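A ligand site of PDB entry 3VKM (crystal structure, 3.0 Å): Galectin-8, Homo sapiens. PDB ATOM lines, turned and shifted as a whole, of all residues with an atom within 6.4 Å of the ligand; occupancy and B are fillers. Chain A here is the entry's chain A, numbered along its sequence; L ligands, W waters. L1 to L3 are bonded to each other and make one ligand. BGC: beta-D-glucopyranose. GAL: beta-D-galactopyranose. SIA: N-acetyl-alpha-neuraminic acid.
Merely in contact with the ligand: Gln 47 (3.6 Å). Hydrophobic or aromatic side chains within 4 Å of the ligand: His 65 and Trp 86. Of the 19 residues printed, 9 come within 4 Å of the ligand. The nearest printed residue that does not touch the ligand is Val 77 (4.6 Å).
The guanidinium group (NH1) of Arg 69 is in hydrogen-bond range of an oxygen (O3) of BGC L1 (2.8 Å). The side-chain amide nitrogen (ND2) of Asn 79 sits at hydrogen-bond distance from an oxygen (O6) of GAL L2, 3.0 Å away. NH1 of Arg 59 is in salt-bridge range of O1A of SIA L3 (2.6 Å). OE2 of Glu 89 is in hydrogen-bond range of O6 of GAL L2 (2.7 Å). A ring nitrogen (NE2) of His 65 lies within hydrogen-bond range of an oxygen (O4) of GAL L2 (2.7 Å). O3 of GAL L2 is in hydrogen-bond range of NH2 of Arg 45. The indole nitrogen of Trp 86 lies within hydrogen-bond range of an oxygen (O1B) of SIA L3. The side-chain amide oxygen (OD1) of Asn 67 is in hydrogen-bond range of an oxygen (O4) of GAL L2 (3.3 Å).
Water W1 bridges O4 of BGC L1 (3.1 Å) and NH2 of Arg 69 (3.2 Å).
The backbone carbonyl oxygen (O) of Gly 87 is in hydrogen-bond range of the side-chain amide nitrogen (ND2) of Asn 79. The guanidinium group of Arg 59 lies within salt-bridge range of the side-chain carboxylate of Asp 49, 3.8 Å away. The backbone NH (N) of His 65 sits at hydrogen-bond distance from the backbone carbonyl oxygen (O) of Asn 79 (2.9 Å). The backbone carbonyl oxygen of Asn 67 is in hydrogen-bond range of the backbone NH of Val 77 (2.8 Å). The side-chain amide oxygen (OD1) of Asn 79 lies close to the backbone carbonyl oxygen (O) of Arg 88 (3.4 Å). The side-chain sulfur (SG) of Cys 78 lies close to the backbone carbonyl oxygen (O) of His 65 (3.8 Å). A ring nitrogen (ND1) of His 65 is in hydrogen-bond range of the side-chain carboxylate (OD2) of Asp 49 (2.6 Å). The backbone NH of Arg 59 is in hydrogen-bond range of the side-chain carboxylate of Glu 84.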
ATOM      1  N   ARG A  45     -32.192  16.678 -28.346  1.00  0.00           N
ATOM      2  CA  ARG A  45     -30.889  16.616 -27.691  1.00  0.00           C
ATOM      3  C   ARG A  45     -30.794  15.444 -26.728  1.00  0.00           C
ATOM      4  O   ARG A  45     -31.800  14.983 -26.208  1.00  0.00           O
ATOM      5  CB  ARG A  45     -30.633  17.915 -26.907  1.00  0.00           C
ATOM      6  CG  ARG A  45     -31.648  18.198 -25.796  1.00  0.00           C
ATOM      7  CD  ARG A  45     -31.070  19.172 -24.766  1.00  0.00           C
ATOM      8  NE  ARG A  45     -30.135  18.517 -23.847  1.00  0.00           N
ATOM      9  CZ  ARG A  45     -29.323  19.167 -23.015  1.00  0.00           C
ATOM     10  NH1 ARG A  45     -29.303  20.504 -22.976  1.00  0.00           N
ATOM     11  NH2 ARG A  45     -28.518  18.478 -22.208  1.00  0.00           N
ATOM     12  N   GLN A  47     -27.669  13.303 -23.912  1.00  0.00           N
ATOM     13  CA  GLN A  47     -26.364  13.450 -23.286  1.00  0.00           C
ATOM     14  C   GLN A  47     -25.784  12.201 -22.641  1.00  0.00           C
ATOM     15  O   GLN A  47     -26.505  11.371 -22.084  1.00  0.00           O
ATOM     16  CB  GLN A  47     -26.442  14.554 -22.226  1.00  0.00           C
ATOM     17  CG  GLN A  47     -27.406  14.239 -21.096  1.00  0.00           C
ATOM     18  CD  GLN A  47     -27.658  15.405 -20.161  1.00  0.00           C
ATOM     19  OE1 GLN A  47     -28.347  16.357 -20.505  1.00  0.00           O
ATOM     20  NE2 GLN A  47     -27.087  15.329 -18.964  1.00  0.00           N
ATOM     21  N   ASP A  49     -23.245  11.264 -19.776  1.00  0.00           N
ATOM     22  CA  ASP A  49     -22.577  11.879 -18.639  1.00  0.00           C
ATOM     23  C   ASP A  49     -21.739  10.945 -17.767  1.00  0.00           C
ATOM     24  O   ASP A  49     -22.260   9.993 -17.175  1.00  0.00           O
ATOM     25  CB  ASP A  49     -23.611  12.588 -17.738  1.00  0.00           C
ATOM     26  CG  ASP A  49     -24.148  13.881 -18.341  1.00  0.00           C
ATOM     27  OD1 ASP A  49     -25.018  14.517 -17.698  1.00  0.00           O
ATOM     28  OD2 ASP A  49     -23.711  14.269 -19.439  1.00  0.00           O
ATOM     29  N   ARG A  59     -27.515  17.268  -7.104  1.00  0.00           N
ATOM     30  CA  ARG A  59     -27.183  16.575  -8.339  1.00  0.00           C
ATOM     31  C   ARG A  59     -25.706  16.209  -8.331  1.00  0.00           C
ATOM     32  O   ARG A  59     -24.849  17.054  -8.093  1.00  0.00           O
ATOM     33  CB  ARG A  59     -27.489  17.451  -9.545  1.00  0.00           C
ATOM     34  CG  ARG A  59     -27.110  16.820 -10.836  1.00  0.00           C
ATOM     35  CD  ARG A  59     -27.544  17.656 -11.992  1.00  0.00           C
ATOM     36  NE  ARG A  59     -27.044  17.097 -13.231  1.00  0.00           N
ATOM     37  CZ  ARG A  59     -27.252  17.645 -14.418  1.00  0.00           C
ATOM     38  NH1 ARG A  59     -27.940  18.770 -14.533  1.00  0.00           N
ATOM     39  NH2 ARG A  59     -26.756  17.066 -15.506  1.00  0.00           N
ATOM     40  N   HIS A  65     -19.478  15.991 -19.536  1.00  0.00           N
ATOM     41  CA  HIS A  65     -20.801  16.150 -20.145  1.00  0.00           C
ATOM     42  C   HIS A  65     -20.669  16.101 -21.655  1.00  0.00           C
ATOM     43  O   HIS A  65     -20.127  17.024 -22.267  1.00  0.00           O
ATOM     44  CB  HIS A  65     -21.389  17.496 -19.688  1.00  0.00           C
ATOM     45  CG  HIS A  65     -22.810  17.733 -20.126  1.00  0.00           C
ATOM     46  ND1 HIS A  65     -23.828  16.863 -19.825  1.00  0.00           N
ATOM     47  CD2 HIS A  65     -23.372  18.774 -20.774  1.00  0.00           C
ATOM     48  CE1 HIS A  65     -24.970  17.357 -20.273  1.00  0.00           C
ATOM     49  NE2 HIS A  65     -24.721  18.514 -20.861  1.00  0.00           N
ATOM     50  N   ASN A  67     -22.857  16.235 -24.734  1.00  0.00           N
ATOM     51  CA  ASN A  67     -24.221  16.626 -25.074  1.00  0.00           C
ATOM     52  C   ASN A  67     -24.492  16.989 -26.529  1.00  0.00           C
ATOM     53  O   ASN A  67     -24.405  18.144 -26.929  1.00  0.00           O
ATOM     54  CB  ASN A  67     -24.606  17.812 -24.182  1.00  0.00           C
ATOM     55  CG  ASN A  67     -25.964  18.414 -24.513  1.00  0.00           C
ATOM     56  OD1 ASN A  67     -26.228  19.555 -24.176  1.00  0.00           O
ATOM     57  ND2 ASN A  67     -26.826  17.638 -25.165  1.00  0.00           N
ATOM     58  N   ARG A  69     -26.442  18.131 -29.537  1.00  0.00           N
ATOM     59  CA  ARG A  69     -27.690  18.875 -29.684  1.00  0.00           C
ATOM     60  C   ARG A  69     -28.021  19.026 -31.153  1.00  0.00           C
ATOM     61  O   ARG A  69     -27.154  19.309 -31.980  1.00  0.00           O
ATOM     62  CB  ARG A  69     -27.564  20.247 -29.039  1.00  0.00           C
ATOM     63  CG  ARG A  69     -27.518  20.200 -27.541  1.00  0.00           C
ATOM     64  CD  ARG A  69     -27.223  21.554 -26.954  1.00  0.00           C
ATOM     65  NE  ARG A  69     -27.254  21.508 -25.508  1.00  0.00           N
ATOM     66  CZ  ARG A  69     -26.978  22.533 -24.716  1.00  0.00           C
ATOM     67  NH1 ARG A  69     -26.647  23.702 -25.243  1.00  0.00           N
ATOM     68  NH2 ARG A  69     -27.032  22.388 -23.398  1.00  0.00           N
ATOM     69  N   VAL A  77     -22.068  19.626 -27.318  1.00  0.00           N
ATOM     70  CA  VAL A  77     -21.734  20.524 -26.227  1.00  0.00           C
ATOM     71  C   VAL A  77     -21.102  19.755 -25.088  1.00  0.00           C
ATOM     72  O   VAL A  77     -21.642  18.775 -24.614  1.00  0.00           O
ATOM     73  CB  VAL A  77     -23.001  21.228 -25.683  1.00  0.00           C
ATOM     74  CG1 VAL A  77     -22.633  22.178 -24.569  1.00  0.00           C
ATOM     75  CG2 VAL A  77     -23.702  21.961 -26.814  1.00  0.00           C
ATOM     76  N   CYS A  78     -19.939  20.220 -24.643  1.00  0.00           N
ATOM     77  CA  CYS A  78     -19.262  19.549 -23.558  1.00  0.00           C
ATOM     78  C   CYS A  78     -18.984  20.498 -22.403  1.00  0.00           C
ATOM     79  O   CYS A  78     -18.625  21.663 -22.617  1.00  0.00           O
ATOM     80  CB  CYS A  78     -17.945  18.947 -24.053  1.00  0.00           C
ATOM     81  SG  CYS A  78     -18.169  17.801 -25.406  1.00  0.00           S
ATOM     82  N   ASN A  79     -19.151  20.000 -21.186  1.00  0.00           N
ATOM     83  CA  ASN A  79     -18.944  20.815 -20.007  1.00  0.00           C
ATOM     84  C   ASN A  79     -18.658  19.909 -18.811  1.00  0.00           C
ATOM     85  O   ASN A  79     -18.480  18.706 -18.962  1.00  0.00           O
ATOM     86  CB  ASN A  79     -20.202  21.654 -19.728  1.00  0.00           C
ATOM     87  CG  ASN A  79     -19.882  22.966 -19.042  1.00  0.00           C
ATOM     88  OD1 ASN A  79     -19.098  23.017 -18.105  1.00  0.00           O
ATOM     89  ND2 ASN A  79     -20.498  24.042 -19.519  1.00  0.00           N
ATOM     90  N   THR A  80     -18.564  20.515 -17.638  1.00  0.00           N
ATOM     91  CA  THR A  80     -18.320  19.783 -16.403  1.00  0.00           C
ATOM     92  C   THR A  80     -19.195  20.394 -15.310  1.00  0.00           C
ATOM     93  O   THR A  80     -19.288  21.625 -15.195  1.00  0.00           O
ATOM     94  CB  THR A  80     -16.843  19.874 -15.988  1.00  0.00           C
ATOM     95  OG1 THR A  80     -16.039  19.227 -16.989  1.00  0.00           O
ATOM     96  CG2 THR A  80     -16.613  19.226 -14.618  1.00  0.00           C
ATOM     97  N   LEU A  81     -19.841  19.563 -14.496  1.00  0.00           N
ATOM     98  CA  LEU A  81     -20.681  20.098 -13.435  1.00  0.00           C
ATOM     99  C   LEU A  81     -20.173  19.795 -12.033  1.00  0.00           C
ATOM    100  O   LEU A  81     -20.176  18.651 -11.601  1.00  0.00           O
ATOM    101  CB  LEU A  81     -22.117  19.615 -13.591  1.00  0.00           C
ATOM    102  CG  LEU A  81     -23.087  20.279 -12.615  1.00  0.00           C
ATOM    103  CD1 LEU A  81     -24.308  20.813 -13.341  1.00  0.00           C
ATOM    104  CD2 LEU A  81     -23.457  19.280 -11.538  1.00  0.00           C
ATOM    105  N   GLU A  84     -23.285  21.250  -8.690  1.00  0.00           N
ATOM    106  CA  GLU A  84     -24.501  21.650  -9.395  1.00  0.00           C
ATOM    107  C   GLU A  84     -24.376  22.924 -10.207  1.00  0.00           C
ATOM    108  O   GLU A  84     -25.389  23.512 -10.597  1.00  0.00           O
ATOM    109  CB  GLU A  84     -25.650  21.780  -8.379  1.00  0.00           C
ATOM    110  CG  GLU A  84     -25.802  20.545  -7.529  1.00  0.00           C
ATOM    111  CD  GLU A  84     -26.810  20.724  -6.437  1.00  0.00           C
ATOM    112  OE1 GLU A  84     -26.636  21.652  -5.620  1.00  0.00           O
ATOM    113  OE2 GLU A  84     -27.778  19.941  -6.385  1.00  0.00           O
ATOM    114  N   TRP A  86     -22.549  24.667 -13.644  1.00  0.00           N
ATOM    115  CA  TRP A  86     -21.843  24.372 -14.893  1.00  0.00           C
ATOM    116  C   TRP A  86     -20.619  25.259 -15.070  1.00  0.00           C
ATOM    117  O   TRP A  86     -20.620  26.429 -14.661  1.00  0.00           O
ATOM    118  CB  TRP A  86     -22.778  24.556 -16.084  1.00  0.00           C
ATOM    119  CG  TRP A  86     -23.803  23.464 -16.251  1.00  0.00           C
ATOM    120  CD1 TRP A  86     -25.156  23.601 -16.196  1.00  0.00           C
ATOM    121  CD2 TRP A  86     -23.547  22.076 -16.514  1.00  0.00           C
ATOM    122  NE1 TRP A  86     -25.765  22.384 -16.417  1.00  0.00           N
ATOM    123  CE2 TRP A  86     -24.801  21.433 -16.606  1.00  0.00           C
ATOM    124  CE3 TRP A  86     -22.374  21.312 -16.675  1.00  0.00           C
ATOM    125  CZ2 TRP A  86     -24.925  20.054 -16.862  1.00  0.00           C
ATOM    126  CZ3 TRP A  86     -22.501  19.947 -16.929  1.00  0.00           C
ATOM    127  CH2 TRP A  86     -23.761  19.331 -17.016  1.00  0.00           C
ATOM    128  N   GLY A  87     -19.557  24.700 -15.658  1.00  0.00           N
ATOM    129  CA  GLY A  87     -18.349  25.449 -15.902  1.00  0.00           C
ATOM    130  C   GLY A  87     -18.413  26.023 -17.301  1.00  0.00           C
ATOM    131  O   GLY A  87     -19.498  26.249 -17.828  1.00  0.00           O
ATOM    132  N   ARG A  88     -17.244  26.250 -17.902  1.00  0.00           N
ATOM    133  CA  ARG A  88     -17.156  26.794 -19.263  1.00  0.00           C
ATOM    134  C   ARG A  88     -17.523  25.730 -20.311  1.00  0.00           C
ATOM    135  O   ARG A  88     -16.999  24.611 -20.277  1.00  0.00           O
ATOM    136  CB  ARG A  88     -15.726  27.288 -19.521  1.00  0.00           C
ATOM    137  CG  ARG A  88     -14.651  26.242 -19.243  1.00  0.00           C
ATOM    138  CD  ARG A  88     -13.286  26.876 -19.022  1.00  0.00           C
ATOM    139  NE  ARG A  88     -12.425  26.052 -18.171  1.00  0.00           N
ATOM    140  CZ  ARG A  88     -11.656  25.056 -18.602  1.00  0.00           C
ATOM    141  NH1 ARG A  88     -11.613  24.741 -19.885  1.00  0.00           N
ATOM    142  NH2 ARG A  88     -10.931  24.362 -17.723  1.00  0.00           N
ATOM    143  N   GLU A  89     -18.454  26.054 -21.207  1.00  0.00           N
ATOM    144  CA  GLU A  89     -18.824  25.116 -22.265  1.00  0.00           C
ATOM    145  C   GLU A  89     -17.754  25.019 -23.345  1.00  0.00           C
ATOM    146  O   GLU A  89     -17.165  26.036 -23.728  1.00  0.00           O
ATOM    147  CB  GLU A  89     -20.143  25.519 -22.930  1.00  0.00           C
ATOM    148  CG  GLU A  89     -21.351  25.503 -22.023  1.00  0.00           C
ATOM    149  CD  GLU A  89     -22.664  25.560 -22.789  1.00  0.00           C
ATOM    150  OE1 GLU A  89     -22.821  26.435 -23.657  1.00  0.00           O
ATOM    151  OE2 GLU A  89     -23.548  24.716 -22.502  1.00  0.00           O
ATOM    152  N   ILE A  91     -17.703  23.793 -27.082  1.00  0.00           N
ATOM    153  CA  ILE A  91     -18.617  23.363 -28.117  1.00  0.00           C
ATOM    154  C   ILE A  91     -17.953  22.978 -29.437  1.00  0.00           C
ATOM    155  O   ILE A  91     -17.130  23.727 -29.966  1.00  0.00           O
ATOM    156  CB  ILE A  91     -19.671  24.457 -28.399  1.00  0.00           C
ATOM    157  CG1 ILE A  91     -20.443  24.770 -27.117  1.00  0.00           C
ATOM    158  CG2 ILE A  91     -20.623  24.004 -29.508  1.00  0.00           C
ATOM    159  CD1 ILE A  91     -21.452  25.886 -27.265  1.00  0.00           C
ATOM    160  N   TYR A 141     -29.028  10.391 -20.944  1.00  0.00           N
ATOM    161  CA  TYR A 141     -30.327  11.049 -20.897  1.00  0.00           C
ATOM    162  C   TYR A 141     -30.692  11.722 -22.212  1.00  0.00           C
ATOM    163  O   TYR A 141     -29.838  11.958 -23.081  1.00  0.00           O
ATOM    164  CB  TYR A 141     -30.334  12.111 -19.807  1.00  0.00           C
ATOM    165  CG  TYR A 141     -29.623  11.698 -18.536  1.00  0.00           C
ATOM    166  CD1 TYR A 141     -30.183  10.748 -17.693  1.00  0.00           C
ATOM    167  CD2 TYR A 141     -28.389  12.252 -18.196  1.00  0.00           C
ATOM    168  CE1 TYR A 141     -29.535  10.356 -16.527  1.00  0.00           C
ATOM    169  CE2 TYR A 141     -27.727  11.878 -17.029  1.00  0.00           C
ATOM    170  CZ  TYR A 141     -28.310  10.924 -16.192  1.00  0.00           C
ATOM    171  OH  TYR A 141     -27.686  10.570 -15.017  1.00  0.00           O
HETATM  172  C2  BGC L   1     -26.136  27.832 -22.480  1.00  0.00           C
HETATM  173  C3  BGC L   1     -26.851  26.481 -22.456  1.00  0.00           C
HETATM  174  C4  BGC L   1     -27.058  26.011 -21.014  1.00  0.00           C
HETATM  175  C5  BGC L   1     -27.729  27.095 -20.172  1.00  0.00           C
HETATM  176  C6  BGC L   1     -27.776  26.729 -18.699  1.00  0.00           C
HETATM  177  C1  BGC L   1     -26.862  28.837 -21.575  1.00  0.00           C
HETATM  178  O1  BGC L   1     -26.137  30.008 -21.515  1.00  0.00           O
HETATM  179  O2  BGC L   1     -26.122  28.315 -23.816  1.00  0.00           O
HETATM  180  O3  BGC L   1     -26.078  25.524 -23.161  1.00  0.00           O
HETATM  181  O4  BGC L   1     -27.867  24.821 -21.012  1.00  0.00           O
HETATM  182  O5  BGC L   1     -26.965  28.324 -20.241  1.00  0.00           O
HETATM  183  O6  BGC L   1     -26.562  27.080 -18.044  1.00  0.00           O
HETATM  184  C1  GAL L   2     -27.442  23.803 -20.171  1.00  0.00           C
HETATM  185  C2  GAL L   2     -28.337  22.596 -20.335  1.00  0.00           C
HETATM  186  C3  GAL L   2     -27.840  21.497 -19.412  1.00  0.00           C
HETATM  187  C4  GAL L   2     -26.393  21.155 -19.754  1.00  0.00           C
HETATM  188  C5  GAL L   2     -25.548  22.424 -19.666  1.00  0.00           C
HETATM  189  C6  GAL L   2     -24.118  22.199 -20.114  1.00  0.00           C
HETATM  190  O2  GAL L   2     -29.671  22.931 -20.001  1.00  0.00           O
HETATM  191  O3  GAL L   2     -28.668  20.328 -19.554  1.00  0.00           O
HETATM  192  O4  GAL L   2     -26.326  20.622 -21.059  1.00  0.00           O
HETATM  193  O5  GAL L   2     -26.089  23.453 -20.523  1.00  0.00           O
HETATM  194  O6  GAL L   2     -23.398  23.413 -20.184  1.00  0.00           O
HETATM  195  C1  SIA L   3     -28.615  19.702 -17.254  1.00  0.00           C
HETATM  196  C2  SIA L   3     -29.484  20.046 -18.464  1.00  0.00           C
HETATM  197  C3  SIA L   3     -30.406  18.833 -18.791  1.00  0.00           C
HETATM  198  C4  SIA L   3     -31.479  18.657 -17.696  1.00  0.00           C
HETATM  199  C5  SIA L   3     -32.193  19.988 -17.504  1.00  0.00           C
HETATM  200  C6  SIA L   3     -31.164  21.004 -17.057  1.00  0.00           C
HETATM  201  C7  SIA L   3     -31.825  22.312 -16.629  1.00  0.00           C
HETATM  202  C8  SIA L   3     -30.906  23.126 -15.705  1.00  0.00           C
HETATM  203  C9  SIA L   3     -30.436  22.321 -14.487  1.00  0.00           C
HETATM  204  C10 SIA L   3     -34.521  19.762 -16.998  1.00  0.00           C
HETATM  205  C11 SIA L   3     -35.085  20.853 -17.900  1.00  0.00           C
HETATM  206  N5  SIA L   3     -33.277  19.908 -16.560  1.00  0.00           N
HETATM  207  O1A SIA L   3     -28.271  18.525 -17.071  1.00  0.00           O
HETATM  208  O1B SIA L   3     -28.264  20.636 -16.490  1.00  0.00           O
HETATM  209  O4  SIA L   3     -32.396  17.651 -18.082  1.00  0.00           O
HETATM  210  O6  SIA L   3     -30.246  21.216 -18.146  1.00  0.00           O
HETATM  211  O7  SIA L   3     -32.137  23.070 -17.789  1.00  0.00           O
HETATM  212  O8  SIA L   3     -29.773  23.591 -16.421  1.00  0.00           O
HETATM  213  O9  SIA L   3     -29.337  22.987 -13.875  1.00  0.00           O
HETATM  214  O10 SIA L   3     -35.215  18.800 -16.708  1.00  0.00           O
HETATM  215  O   HOH W   1     -29.469  24.484 -23.597  1.00  0.00           O
HETATM  216  O   HOH W   2     -30.991  25.145 -19.999  1.00  0.00           O
